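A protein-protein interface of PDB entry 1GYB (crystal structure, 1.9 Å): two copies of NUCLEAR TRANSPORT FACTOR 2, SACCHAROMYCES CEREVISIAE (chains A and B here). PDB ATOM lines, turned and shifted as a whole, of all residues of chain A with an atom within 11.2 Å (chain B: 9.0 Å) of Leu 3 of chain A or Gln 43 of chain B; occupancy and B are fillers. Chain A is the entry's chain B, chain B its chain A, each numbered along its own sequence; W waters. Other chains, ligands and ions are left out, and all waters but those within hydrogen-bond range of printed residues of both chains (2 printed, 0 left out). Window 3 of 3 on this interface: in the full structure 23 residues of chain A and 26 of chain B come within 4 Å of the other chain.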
ATOM      1  N   LEU A   3      -7.041 -22.693  35.752  1.00  0.00           N
ATOM      2  CA  LEU A   3      -5.632 -22.595  36.221  1.00  0.00           C
ATOM      3  C   LEU A   3      -5.571 -21.553  37.331  1.00  0.00           C
ATOM      4  O   LEU A   3      -6.561 -21.307  38.022  1.00  0.00           O
ATOM      5  CB  LEU A   3      -4.717 -22.187  35.061  1.00  0.00           C
ATOM      6  CG  LEU A   3      -3.218 -22.180  35.367  1.00  0.00           C
ATOM      7  CD1 LEU A   3      -2.687 -23.600  35.277  1.00  0.00           C
ATOM      8  CD2 LEU A   3      -2.469 -21.272  34.401  1.00  0.00           C
ATOM      9  N   ASP A   4      -4.401 -20.952  37.511  1.00  0.00           N
ATOM     10  CA  ASP A   4      -4.216 -19.916  38.516  1.00  0.00           C
ATOM     11  C   ASP A   4      -4.209 -18.596  37.753  1.00  0.00           C
ATOM     12  O   ASP A   4      -5.075 -17.748  37.962  1.00  0.00           O
ATOM     13  CB  ASP A   4      -2.886 -20.116  39.256  1.00  0.00           C
ATOM     14  CG  ASP A   4      -2.714 -19.160  40.427  1.00  0.00           C
ATOM     15  OD1 ASP A   4      -3.460 -19.281  41.428  1.00  0.00           O
ATOM     16  OD2 ASP A   4      -1.826 -18.278  40.356  1.00  0.00           O
ATOM     17  N   PHE A   5      -3.238 -18.440  36.854  1.00  0.00           N
ATOM     18  CA  PHE A   5      -3.135 -17.227  36.052  1.00  0.00           C
ATOM     19  C   PHE A   5      -4.343 -17.082  35.137  1.00  0.00           C
ATOM     20  O   PHE A   5      -4.743 -15.962  34.811  1.00  0.00           O
ATOM     21  CB  PHE A   5      -1.831 -17.219  35.239  1.00  0.00           C
ATOM     22  CG  PHE A   5      -0.601 -17.065  36.086  1.00  0.00           C
ATOM     23  CD1 PHE A   5       0.014 -18.174  36.653  1.00  0.00           C
ATOM     24  CD2 PHE A   5      -0.096 -15.801  36.375  1.00  0.00           C
ATOM     25  CE1 PHE A   5       1.109 -18.028  37.496  1.00  0.00           C
ATOM     26  CE2 PHE A   5       1.001 -15.645  37.220  1.00  0.00           C
ATOM     27  CZ  PHE A   5       1.604 -16.762  37.784  1.00  0.00           C
ATOM     28  N   ASN A   6      -4.930 -18.203  34.720  1.00  0.00           N
ATOM     29  CA  ASN A   6      -6.117 -18.129  33.877  1.00  0.00           C
ATOM     30  C   ASN A   6      -7.299 -17.692  34.744  1.00  0.00           C
ATOM     31  O   ASN A   6      -8.151 -16.933  34.294  1.00  0.00           O
ATOM     32  CB  ASN A   6      -6.417 -19.475  33.199  1.00  0.00           C
ATOM     33  CG  ASN A   6      -5.558 -19.713  31.958  1.00  0.00           C
ATOM     34  OD1 ASN A   6      -5.129 -18.766  31.295  1.00  0.00           O
ATOM     35  ND2 ASN A   6      -5.322 -20.979  31.629  1.00  0.00           N
ATOM     36  N   THR A   7      -7.333 -18.164  35.988  1.00  0.00           N
ATOM     37  CA  THR A   7      -8.400 -17.805  36.917  1.00  0.00           C
ATOM     38  C   THR A   7      -8.213 -16.367  37.392  1.00  0.00           C
ATOM     39  O   THR A   7      -9.181 -15.613  37.515  1.00  0.00           O
ATOM     40  CB  THR A   7      -8.423 -18.745  38.141  1.00  0.00           C
ATOM     41  OG1 THR A   7      -8.792 -20.064  37.717  1.00  0.00           O
ATOM     42  CG2 THR A   7      -9.428 -18.257  39.180  1.00  0.00           C
ATOM     43  N   LEU A   8      -6.964 -15.996  37.659  1.00  0.00           N
ATOM     44  CA  LEU A   8      -6.647 -14.641  38.100  1.00  0.00           C
ATOM     45  C   LEU A   8      -6.993 -13.675  36.967  1.00  0.00           C
ATOM     46  O   LEU A   8      -7.631 -12.639  37.184  1.00  0.00           O
ATOM     47  CB  LEU A   8      -5.153 -14.527  38.449  1.00  0.00           C
ATOM     48  CG  LEU A   8      -4.618 -15.451  39.549  1.00  0.00           C
ATOM     49  CD1 LEU A   8      -3.112 -15.262  39.690  1.00  0.00           C
ATOM     50  CD2 LEU A   8      -5.317 -15.160  40.870  1.00  0.00           C
ATOM     51  N   ALA A   9      -6.570 -14.029  35.756  1.00  0.00           N
ATOM     52  CA  ALA A   9      -6.827 -13.209  34.580  1.00  0.00           C
ATOM     53  C   ALA A   9      -8.320 -13.141  34.293  1.00  0.00           C
ATOM     54  O   ALA A   9      -8.852 -12.074  33.986  1.00  0.00           O
ATOM     55  CB  ALA A   9      -6.087 -13.775  33.367  1.00  0.00           C
ATOM     56  N   GLN A  10      -8.993 -14.285  34.389  1.00  0.00           N
ATOM     57  CA  GLN A  10     -10.425 -14.334  34.131  1.00  0.00           C
ATOM     58  C   GLN A  10     -11.181 -13.456  35.114  1.00  0.00           C
ATOM     59  O   GLN A  10     -12.041 -12.677  34.711  1.00  0.00           O
ATOM     60  CB  GLN A  10     -10.962 -15.763  34.230  1.00  0.00           C
ATOM     61  CG  GLN A  10     -12.407 -15.866  33.758  1.00  0.00           C
ATOM     62  CD  GLN A  10     -13.008 -17.248  33.922  1.00  0.00           C
ATOM     63  OE1 GLN A  10     -14.067 -17.541  33.365  1.00  0.00           O
ATOM     64  NE2 GLN A  10     -12.345 -18.102  34.695  1.00  0.00           N
ATOM     65  N   ASN A  11     -10.866 -13.587  36.400  1.00  0.00           N
ATOM     66  CA  ASN A  11     -11.533 -12.780  37.414  1.00  0.00           C
ATOM     67  C   ASN A  11     -11.539 -11.318  36.985  1.00  0.00           C
ATOM     68  O   ASN A  11     -12.598 -10.690  36.895  1.00  0.00           O
ATOM     69  CB  ASN A  11     -10.829 -12.892  38.772  1.00  0.00           C
ATOM     70  CG  ASN A  11     -11.025 -14.242  39.428  1.00  0.00           C
ATOM     71  OD1 ASN A  11     -11.930 -14.995  39.067  1.00  0.00           O
ATOM     72  ND2 ASN A  11     -10.186 -14.549  40.414  1.00  0.00           N
ATOM     73  N   LEU A  69      -9.717 -17.723  26.496  1.00  0.00           N
ATOM     74  CA  LEU A  69      -8.957 -16.823  27.340  1.00  0.00           C
ATOM     75  C   LEU A  69      -7.736 -17.603  27.793  1.00  0.00           C
ATOM     76  O   LEU A  69      -7.854 -18.690  28.368  1.00  0.00           O
ATOM     77  CB  LEU A  69      -9.787 -16.368  28.545  1.00  0.00           C
ATOM     78  CG  LEU A  69      -9.121 -15.380  29.512  1.00  0.00           C
ATOM     79  CD1 LEU A  69     -10.195 -14.551  30.219  1.00  0.00           C
ATOM     80  CD2 LEU A  69      -8.258 -16.144  30.522  1.00  0.00           C
ATOM     81  N   ASP A  70      -6.563 -17.046  27.513  1.00  0.00           N
ATOM     82  CA  ASP A  70      -5.311 -17.684  27.886  1.00  0.00           C
ATOM     83  C   ASP A  70      -4.405 -16.668  28.544  1.00  0.00           C
ATOM     84  O   ASP A  70      -4.218 -15.569  28.024  1.00  0.00           O
ATOM     85  CB  ASP A  70      -4.643 -18.259  26.640  1.00  0.00           C
ATOM     86  CG  ASP A  70      -5.492 -19.320  25.978  1.00  0.00           C
ATOM     87  OD1 ASP A  70      -5.665 -20.402  26.581  1.00  0.00           O
ATOM     88  OD2 ASP A  70      -5.996 -19.072  24.865  1.00  0.00           O
ATOM     89  N   ALA A  71      -3.836 -17.038  29.687  1.00  0.00           N
ATOM     90  CA  ALA A  71      -2.964 -16.129  30.409  1.00  0.00           C
ATOM     91  C   ALA A  71      -1.643 -16.750  30.840  1.00  0.00           C
ATOM     92  O   ALA A  71      -1.517 -17.970  30.978  1.00  0.00           O
ATOM     93  CB  ALA A  71      -3.693 -15.580  31.623  1.00  0.00           C
ATOM     94  N   GLN A  72      -0.658 -15.885  31.049  1.00  0.00           N
ATOM     95  CA  GLN A  72       0.673 -16.293  31.484  1.00  0.00           C
ATOM     96  C   GLN A  72       1.247 -15.162  32.312  1.00  0.00           C
ATOM     97  O   GLN A  72       0.843 -14.011  32.169  1.00  0.00           O
ATOM     98  CB  GLN A  72       1.626 -16.492  30.294  1.00  0.00           C
ATOM     99  CG  GLN A  72       1.336 -17.644  29.349  1.00  0.00           C
ATOM    100  CD  GLN A  72       2.400 -17.765  28.256  1.00  0.00           C
ATOM    101  OE1 GLN A  72       3.165 -16.830  28.011  1.00  0.00           O
ATOM    102  NE2 GLN A  72       2.444 -18.912  27.591  1.00  0.00           N
ATOM    103  N   PRO A  73       2.191 -15.474  33.209  1.00  0.00           N
ATOM    104  CA  PRO A  73       2.758 -14.366  33.984  1.00  0.00           C
ATOM    105  C   PRO A  73       3.608 -13.598  32.969  1.00  0.00           C
ATOM    106  O   PRO A  73       4.357 -14.209  32.204  1.00  0.00           O
ATOM    107  CB  PRO A  73       3.595 -15.077  35.046  1.00  0.00           C
ATOM    108  CG  PRO A  73       3.952 -16.382  34.405  1.00  0.00           C
ATOM    109  CD  PRO A  73       2.681 -16.776  33.693  1.00  0.00           C
ATOM    110  N   ALA A  74       3.478 -12.275  32.942  1.00  0.00           N
ATOM    111  CA  ALA A  74       4.216 -11.464  31.973  1.00  0.00           C
ATOM    112  C   ALA A  74       5.674 -11.258  32.364  1.00  0.00           C
ATOM    113  O   ALA A  74       6.493 -10.827  31.553  1.00  0.00           O
ATOM    114  CB  ALA A  74       3.520 -10.116  31.784  1.00  0.00           C
ATOM    115  N   VAL A  80       0.498  -9.781  34.582  1.00  0.00           N
ATOM    116  CA  VAL A  80      -0.067 -10.870  33.807  1.00  0.00           C
ATOM    117  C   VAL A  80      -0.383 -10.476  32.374  1.00  0.00           C
ATOM    118  O   VAL A  80      -0.765  -9.341  32.104  1.00  0.00           O
ATOM    119  CB  VAL A  80      -1.368 -11.379  34.485  1.00  0.00           C
ATOM    120  CG1 VAL A  80      -1.962 -12.529  33.691  1.00  0.00           C
ATOM    121  CG2 VAL A  80      -1.070 -11.814  35.923  1.00  0.00           C
ATOM    122  N   LEU A  81      -0.209 -11.429  31.466  1.00  0.00           N
ATOM    123  CA  LEU A  81      -0.506 -11.220  30.052  1.00  0.00           C
ATOM    124  C   LEU A  81      -1.667 -12.159  29.731  1.00  0.00           C
ATOM    125  O   LEU A  81      -1.622 -13.344  30.061  1.00  0.00           O
ATOM    126  CB  LEU A  81       0.701 -11.589  29.186  1.00  0.00           C
ATOM    127  CG  LEU A  81       0.573 -11.354  27.679  1.00  0.00           C
ATOM    128  CD1 LEU A  81       0.498  -9.867  27.412  1.00  0.00           C
ATOM    129  CD2 LEU A  81       1.774 -11.971  26.953  1.00  0.00           C
ATOM    130  N   VAL A  82      -2.710 -11.631  29.103  1.00  0.00           N
ATOM    131  CA  VAL A  82      -3.859 -12.452  28.759  1.00  0.00           C
ATOM    132  C   VAL A  82      -4.299 -12.163  27.334  1.00  0.00           C
ATOM    133  O   VAL A  82      -4.309 -11.006  26.902  1.00  0.00           O
ATOM    134  CB  VAL A  82      -5.038 -12.172  29.730  1.00  0.00           C
ATOM    135  CG1 VAL A  82      -5.326 -10.682  29.774  1.00  0.00           C
ATOM    136  CG2 VAL A  82      -6.284 -12.946  29.296  1.00  0.00           C
ATOM    137  N   TYR A 112      -6.064  -5.218  39.566  1.00  0.00           N
ATOM    138  CA  TYR A 112      -5.074  -4.826  38.570  1.00  0.00           C
ATOM    139  C   TYR A 112      -5.553  -3.602  37.820  1.00  0.00           C
ATOM    140  O   TYR A 112      -6.693  -3.167  37.972  1.00  0.00           O
ATOM    141  CB  TYR A 112      -4.889  -5.914  37.507  1.00  0.00           C
ATOM    142  CG  TYR A 112      -4.478  -7.278  37.999  1.00  0.00           C
ATOM    143  CD1 TYR A 112      -5.414  -8.162  38.535  1.00  0.00           C
ATOM    144  CD2 TYR A 112      -3.156  -7.695  37.903  1.00  0.00           C
ATOM    145  CE1 TYR A 112      -5.039  -9.430  38.963  1.00  0.00           C
ATOM    146  CE2 TYR A 112      -2.768  -8.958  38.324  1.00  0.00           C
ATOM    147  CZ  TYR A 112      -3.712  -9.821  38.852  1.00  0.00           C
ATOM    148  OH  TYR A 112      -3.330 -11.076  39.252  1.00  0.00           O
ATOM    149  N   SER B  35      11.287 -19.001  29.236  1.00  0.00           N
ATOM    150  CA  SER B  35      10.236 -18.843  28.231  1.00  0.00           C
ATOM    151  C   SER B  35       9.049 -19.771  28.412  1.00  0.00           C
ATOM    152  O   SER B  35       9.200 -20.931  28.793  1.00  0.00           O
ATOM    153  CB  SER B  35      10.830 -19.026  26.837  1.00  0.00           C
ATOM    154  OG  SER B  35      11.788 -18.008  26.587  1.00  0.00           O
ATOM    155  N   MET B  36       7.862 -19.253  28.112  1.00  0.00           N
ATOM    156  CA  MET B  36       6.633 -20.022  28.249  1.00  0.00           C
ATOM    157  C   MET B  36       5.808 -19.992  26.974  1.00  0.00           C
ATOM    158  O   MET B  36       5.624 -18.937  26.363  1.00  0.00           O
ATOM    159  CB  MET B  36       5.786 -19.453  29.388  1.00  0.00           C
ATOM    160  CG  MET B  36       6.453 -19.487  30.754  1.00  0.00           C
ATOM    161  SD  MET B  36       5.595 -18.408  31.917  1.00  0.00           S
ATOM    162  CE  MET B  36       6.396 -16.836  31.580  1.00  0.00           C
ATOM    163  N   LEU B  37       5.314 -21.162  26.585  1.00  0.00           N
ATOM    164  CA  LEU B  37       4.474 -21.293  25.402  1.00  0.00           C
ATOM    165  C   LEU B  37       3.151 -21.932  25.777  1.00  0.00           C
ATOM    166  O   LEU B  37       3.110 -22.982  26.421  1.00  0.00           O
ATOM    167  CB  LEU B  37       5.138 -22.174  24.335  1.00  0.00           C
ATOM    168  CG  LEU B  37       4.184 -22.682  23.238  1.00  0.00           C
ATOM    169  CD1 LEU B  37       3.725 -21.527  22.351  1.00  0.00           C
ATOM    170  CD2 LEU B  37       4.871 -23.751  22.397  1.00  0.00           C
ATOM    171  N   THR B  38       2.066 -21.276  25.400  1.00  0.00           N
ATOM    172  CA  THR B  38       0.753 -21.841  25.631  1.00  0.00           C
ATOM    173  C   THR B  38       0.292 -22.085  24.215  1.00  0.00           C
ATOM    174  O   THR B  38      -0.025 -21.142  23.483  1.00  0.00           O
ATOM    175  CB  THR B  38      -0.209 -20.856  26.301  1.00  0.00           C
ATOM    176  OG1 THR B  38       0.231 -20.598  27.637  1.00  0.00           O
ATOM    177  CG2 THR B  38      -1.619 -21.439  26.335  1.00  0.00           C
ATOM    178  N   PHE B  39       0.324 -23.345  23.805  1.00  0.00           N
ATOM    179  CA  PHE B  39      -0.105 -23.703  22.469  1.00  0.00           C
ATOM    180  C   PHE B  39      -1.468 -24.333  22.664  1.00  0.00           C
ATOM    181  O   PHE B  39      -1.585 -25.526  22.947  1.00  0.00           O
ATOM    182  CB  PHE B  39       0.858 -24.702  21.833  1.00  0.00           C
ATOM    183  CG  PHE B  39       0.605 -24.929  20.373  1.00  0.00           C
ATOM    184  CD1 PHE B  39       1.247 -24.156  19.415  1.00  0.00           C
ATOM    185  CD2 PHE B  39      -0.300 -25.900  19.953  1.00  0.00           C
ATOM    186  CE1 PHE B  39       0.995 -24.347  18.050  1.00  0.00           C
ATOM    187  CE2 PHE B  39      -0.561 -26.098  18.600  1.00  0.00           C
ATOM    188  CZ  PHE B  39       0.089 -25.318  17.645  1.00  0.00           C
ATOM    189  N   GLU B  40      -2.498 -23.506  22.521  1.00  0.00           N
ATOM    190  CA  GLU B  40      -3.866 -23.947  22.717  1.00  0.00           C
ATOM    191  C   GLU B  40      -3.964 -24.546  24.123  1.00  0.00           C
ATOM    192  O   GLU B  40      -3.824 -23.811  25.100  1.00  0.00           O
ATOM    193  CB  GLU B  40      -4.254 -24.932  21.613  1.00  0.00           C
ATOM    194  CG  GLU B  40      -4.072 -24.300  20.229  1.00  0.00           C
ATOM    195  CD  GLU B  40      -4.953 -24.900  19.155  1.00  0.00           C
ATOM    196  OE1 GLU B  40      -4.608 -25.977  18.612  1.00  0.00           O
ATOM    197  OE2 GLU B  40      -6.005 -24.293  18.848  1.00  0.00           O
ATOM    198  N   THR B  41      -4.177 -25.851  24.258  1.00  0.00           N
ATOM    199  CA  THR B  41      -4.274 -26.413  25.606  1.00  0.00           C
ATOM    200  C   THR B  41      -2.950 -26.918  26.183  1.00  0.00           C
ATOM    201  O   THR B  41      -2.902 -27.357  27.335  1.00  0.00           O
ATOM    202  CB  THR B  41      -5.320 -27.555  25.675  1.00  0.00           C
ATOM    203  OG1 THR B  41      -5.058 -28.520  24.649  1.00  0.00           O
ATOM    204  CG2 THR B  41      -6.726 -26.998  25.499  1.00  0.00           C
ATOM    205  N   SER B  42      -1.878 -26.845  25.399  1.00  0.00           N
ATOM    206  CA  SER B  42      -0.564 -27.299  25.857  1.00  0.00           C
ATOM    207  C   SER B  42       0.235 -26.154  26.477  1.00  0.00           C
ATOM    208  O   SER B  42       0.369 -25.086  25.879  1.00  0.00           O
ATOM    209  CB  SER B  42       0.238 -27.883  24.691  1.00  0.00           C
ATOM    210  OG  SER B  42      -0.400 -29.009  24.118  1.00  0.00           O
ATOM    211  N   GLN B  43       0.769 -26.384  27.673  1.00  0.00           N
ATOM    212  CA  GLN B  43       1.566 -25.374  28.359  1.00  0.00           C
ATOM    213  C   GLN B  43       2.998 -25.878  28.536  1.00  0.00           C
ATOM    214  O   GLN B  43       3.231 -26.870  29.225  1.00  0.00           O
ATOM    215  CB  GLN B  43       0.939 -25.046  29.714  1.00  0.00           C
ATOM    216  CG  GLN B  43      -0.315 -24.169  29.611  1.00  0.00           C
ATOM    217  CD  GLN B  43      -1.078 -24.059  30.920  1.00  0.00           C
ATOM    218  OE1 GLN B  43      -0.516 -23.708  31.961  1.00  0.00           O
ATOM    219  NE2 GLN B  43      -2.372 -24.354  30.871  1.00  0.00           N
ATOM    220  N   LEU B  44       3.951 -25.204  27.901  1.00  0.00           N
ATOM    221  CA  LEU B  44       5.350 -25.610  27.995  1.00  0.00           C
ATOM    222  C   LEU B  44       6.255 -24.480  28.486  1.00  0.00           C
ATOM    223  O   LEU B  44       5.940 -23.301  28.314  1.00  0.00           O
ATOM    224  CB  LEU B  44       5.865 -26.106  26.631  1.00  0.00           C
ATOM    225  CG  LEU B  44       5.210 -27.324  25.972  1.00  0.00           C
ATOM    226  CD1 LEU B  44       5.023 -28.433  26.994  1.00  0.00           C
ATOM    227  CD2 LEU B  44       3.880 -26.930  25.367  1.00  0.00           C
ATOM    228  N   GLN B  45       7.374 -24.849  29.112  1.00  0.00           N
ATOM    229  CA  GLN B  45       8.348 -23.874  29.596  1.00  0.00           C
ATOM    230  C   GLN B  45       9.761 -24.333  29.238  1.00  0.00           C
ATOM    231  O   GLN B  45      10.114 -25.494  29.444  1.00  0.00           O
ATOM    232  CB  GLN B  45       8.225 -23.686  31.111  1.00  0.00           C
ATOM    233  CG  GLN B  45       9.114 -22.583  31.686  1.00  0.00           C
ATOM    234  CD  GLN B  45       8.599 -22.092  33.027  1.00  0.00           C
ATOM    235  OE1 GLN B  45       7.928 -22.831  33.745  1.00  0.00           O
ATOM    236  NE2 GLN B  45       8.913 -20.846  33.373  1.00  0.00           N
ATOM    237  N   GLY B  46      10.559 -23.415  28.695  1.00  0.00           N
ATOM    238  CA  GLY B  46      11.929 -23.727  28.308  1.00  0.00           C
ATOM    239  C   GLY B  46      12.047 -24.029  26.825  1.00  0.00           C
ATOM    240  O   GLY B  46      11.164 -24.667  26.262  1.00  0.00           O
ATOM    241  N   ASP B  49      11.414 -27.957  25.622  1.00  0.00           N
ATOM    242  CA  ASP B  49      10.027 -28.407  25.593  1.00  0.00           C
ATOM    243  C   ASP B  49       9.178 -27.638  24.588  1.00  0.00           C
ATOM    244  O   ASP B  49       8.289 -28.208  23.962  1.00  0.00           O
ATOM    245  CB  ASP B  49       9.404 -28.290  26.980  1.00  0.00           C
ATOM    246  CG  ASP B  49      10.023 -29.247  27.979  1.00  0.00           C
ATOM    247  OD1 ASP B  49      10.800 -30.135  27.560  1.00  0.00           O
ATOM    248  OD2 ASP B  49       9.722 -29.116  29.184  1.00  0.00           O
ATOM    249  N   ILE B  50       9.454 -26.347  24.439  1.00  0.00           N
ATOM    250  CA  ILE B  50       8.714 -25.509  23.500  1.00  0.00           C
ATOM    251  C   ILE B  50       8.970 -25.973  22.065  1.00  0.00           C
ATOM    252  O   ILE B  50       8.036 -26.210  21.305  1.00  0.00           O
ATOM    253  CB  ILE B  50       9.117 -24.018  23.665  1.00  0.00           C
ATOM    254  CG1 ILE B  50       8.571 -23.489  24.996  1.00  0.00           C
ATOM    255  CG2 ILE B  50       8.610 -23.186  22.492  1.00  0.00           C
ATOM    256  CD1 ILE B  50       8.973 -22.045  25.309  1.00  0.00           C
ATOM    257  N   LYS B  53       7.326 -29.325  21.291  1.00  0.00           N
ATOM    258  CA  LYS B  53       5.901 -29.233  21.008  1.00  0.00           C
ATOM    259  C   LYS B  53       5.665 -28.796  19.569  1.00  0.00           C
ATOM    260  O   LYS B  53       4.851 -29.385  18.861  1.00  0.00           O
ATOM    261  CB  LYS B  53       5.234 -28.247  21.978  1.00  0.00           C
ATOM    262  CG  LYS B  53       3.764 -27.934  21.664  1.00  0.00           C
ATOM    263  CD  LYS B  53       2.876 -29.180  21.689  1.00  0.00           C
ATOM    264  CE  LYS B  53       1.457 -28.838  21.263  1.00  0.00           C
ATOM    265  NZ  LYS B  53       0.561 -30.035  21.227  1.00  0.00           N
ATOM    266  N   ASP B 117       4.693 -16.565  24.837  1.00  0.00           N
ATOM    267  CA  ASP B 117       4.194 -16.964  23.532  1.00  0.00           C
ATOM    268  C   ASP B 117       2.834 -17.613  23.788  1.00  0.00           C
ATOM    269  O   ASP B 117       2.767 -18.686  24.386  1.00  0.00           O
ATOM    270  CB  ASP B 117       5.135 -17.985  22.888  1.00  0.00           C
ATOM    271  CG  ASP B 117       4.700 -18.380  21.489  1.00  0.00           C
ATOM    272  OD1 ASP B 117       3.516 -18.163  21.138  1.00  0.00           O
ATOM    273  OD2 ASP B 117       5.542 -18.923  20.737  1.00  0.00           O
ATOM    274  N   ILE B 118       1.756 -16.955  23.371  1.00  0.00           N
ATOM    275  CA  ILE B 118       0.412 -17.513  23.551  1.00  0.00           C
ATOM    276  C   ILE B 118      -0.183 -17.664  22.154  1.00  0.00           C
ATOM    277  O   ILE B 118      -0.280 -16.694  21.408  1.00  0.00           O
ATOM    278  CB  ILE B 118      -0.486 -16.592  24.425  1.00  0.00           C
ATOM    279  CG1 ILE B 118       0.175 -16.371  25.799  1.00  0.00           C
ATOM    280  CG2 ILE B 118      -1.864 -17.247  24.624  1.00  0.00           C
ATOM    281  CD1 ILE B 118      -0.601 -15.448  26.750  1.00  0.00           C
ATOM    282  N   ARG B 120      -3.349 -19.517  19.641  1.00  0.00           N
ATOM    283  CA  ARG B 120      -4.672 -20.120  19.565  1.00  0.00           C
ATOM    284  C   ARG B 120      -5.243 -20.123  18.155  1.00  0.00           C
ATOM    285  O   ARG B 120      -5.050 -19.171  17.391  1.00  0.00           O
ATOM    286  CB  ARG B 120      -5.653 -19.351  20.459  1.00  0.00           C
ATOM    287  CG  ARG B 120      -5.685 -19.784  21.897  1.00  0.00           C
ATOM    288  CD  ARG B 120      -6.567 -21.005  22.058  1.00  0.00           C
ATOM    289  NE  ARG B 120      -6.589 -21.476  23.434  1.00  0.00           N
ATOM    290  CZ  ARG B 120      -7.292 -22.522  23.847  1.00  0.00           C
ATOM    291  NH1 ARG B 120      -8.031 -23.204  22.982  1.00  0.00           N
ATOM    292  NH2 ARG B 120      -7.252 -22.888  25.123  1.00  0.00           N
HETATM  293  O   HOH W   1      -7.988 -21.697  28.148  1.00  0.00           O
HETATM  294  O   HOH W   2      -1.880 -20.010  29.271  1.00  0.00           O
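The side-chain amide nitrogen (NE2) of Gln 72 of chain A is in hydrogen-bond range of the backbone carbonyl oxygen (O) of Met 36 of chain B, 3.4 Å away.
OG1 of Thr 38 of chain B is in hydrogen-bond range of NE2 of Gln 72 of chain A.
The side-chain amide nitrogen (NE2) of Gln 72 of chain A lies within hydrogen-bond range of the backbone carbonyl oxygen (O) of Asp 117 of chain B (3.2 Å).
NE of Arg 120 of chain B lies within salt-bridge range of OD2 of Asp 70 of chain A (2.9 Å).
O of Met 36 of chain B sits at hydrogen-bond distance from N of Asp 117 of chain B (3.0 Å).
The backbone carbonyl oxygen (O) of Leu 37 of chain B is in hydrogen-bond range of the backbone NH (N) of Leu 44 of chain B, at 2.8 Å.
The backbone NH of Thr 38 of chain B is in hydrogen-bond range of the backbone carbonyl oxygen of Asp 117 of chain B.
The side-chain hydroxyl of Thr 7 of chain A lies within hydrogen-bond range of the backbone carbonyl oxygen of Leu 3 of chain A.
N of Leu 81 of chain A sits at hydrogen-bond distance from O of Gln 72 of chain A (2.9 Å).
No position is printed for both chains.
Of the 9 pairs that touch across the chains among the printed residues, none has its exchanged pair printed and touching as well.
Leu 3 of chain A touches one residue of chain B.
Ser 35 of chain B touches none of the printed residues of chain A.
Of the printed residues of chain A, Leu 37 of chain B touches Gln 72.
Printed residues of chain A within 4 Å of Thr 38 of chain B: Gln 72 (2.8 Å).
No residue of chain A comes within 4 Å of Ser 42 of chain B.
Gln 43 of chain B touches one residue of chain A.
Of the printed residues of chain A, Ile 118 of chain B touches Asp 70 and Gln 72.
The nearest residue of chain B that does not touch Leu 3 of chain A is Thr 38 of chain B (7.3 Å).
The nearest residue of chain A that does not touch Gln 43 of chain B is Asn 6 of chain A (4.5 Å).
The nearest printed residue of chain B that does not touch Asp 70 of chain A is Glu 40 of chain B (4.1 Å).
Water W2 bridges O of Ala 71 of chain A and OG1 of Thr 38 of chain B.
Water W1 lies within hydrogen-bond range of the backbone carbonyl oxygen (O) of Leu 69 of chain A, the side-chain carboxylate (OD1) of Asp 70 of chain A and the guanidinium group (NH2) of Arg 120 of chain B.
Gln 43 of chain B touches Leu 3 of chain A.
Ile 118 of chain B touches Asp 70 of chain A.
Leu 37 of chain B touches Gln 72 of chain A (C to NE2, 3.6 Å).
Gln 72 of chain A touches Ile 118 of chain B (CD to CG1, 3.6 Å).
O of Pro 73 of chain A touches CE of Met 36 of chain B, at 3.4 Å.
Of the 18 printed residues of chain B, 7 touch a printed residue of chain A.
Printed residues of chain B that touch a printed residue of chain A: Met 36, Leu 37, Thr 38, Gln 43, Asp 117, Ile 118 and Arg 120.
Of the 19 printed residues of chain A, 4 touch a printed residue of chain B.
Among the printed residues, 9 pairs touch across the chains.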
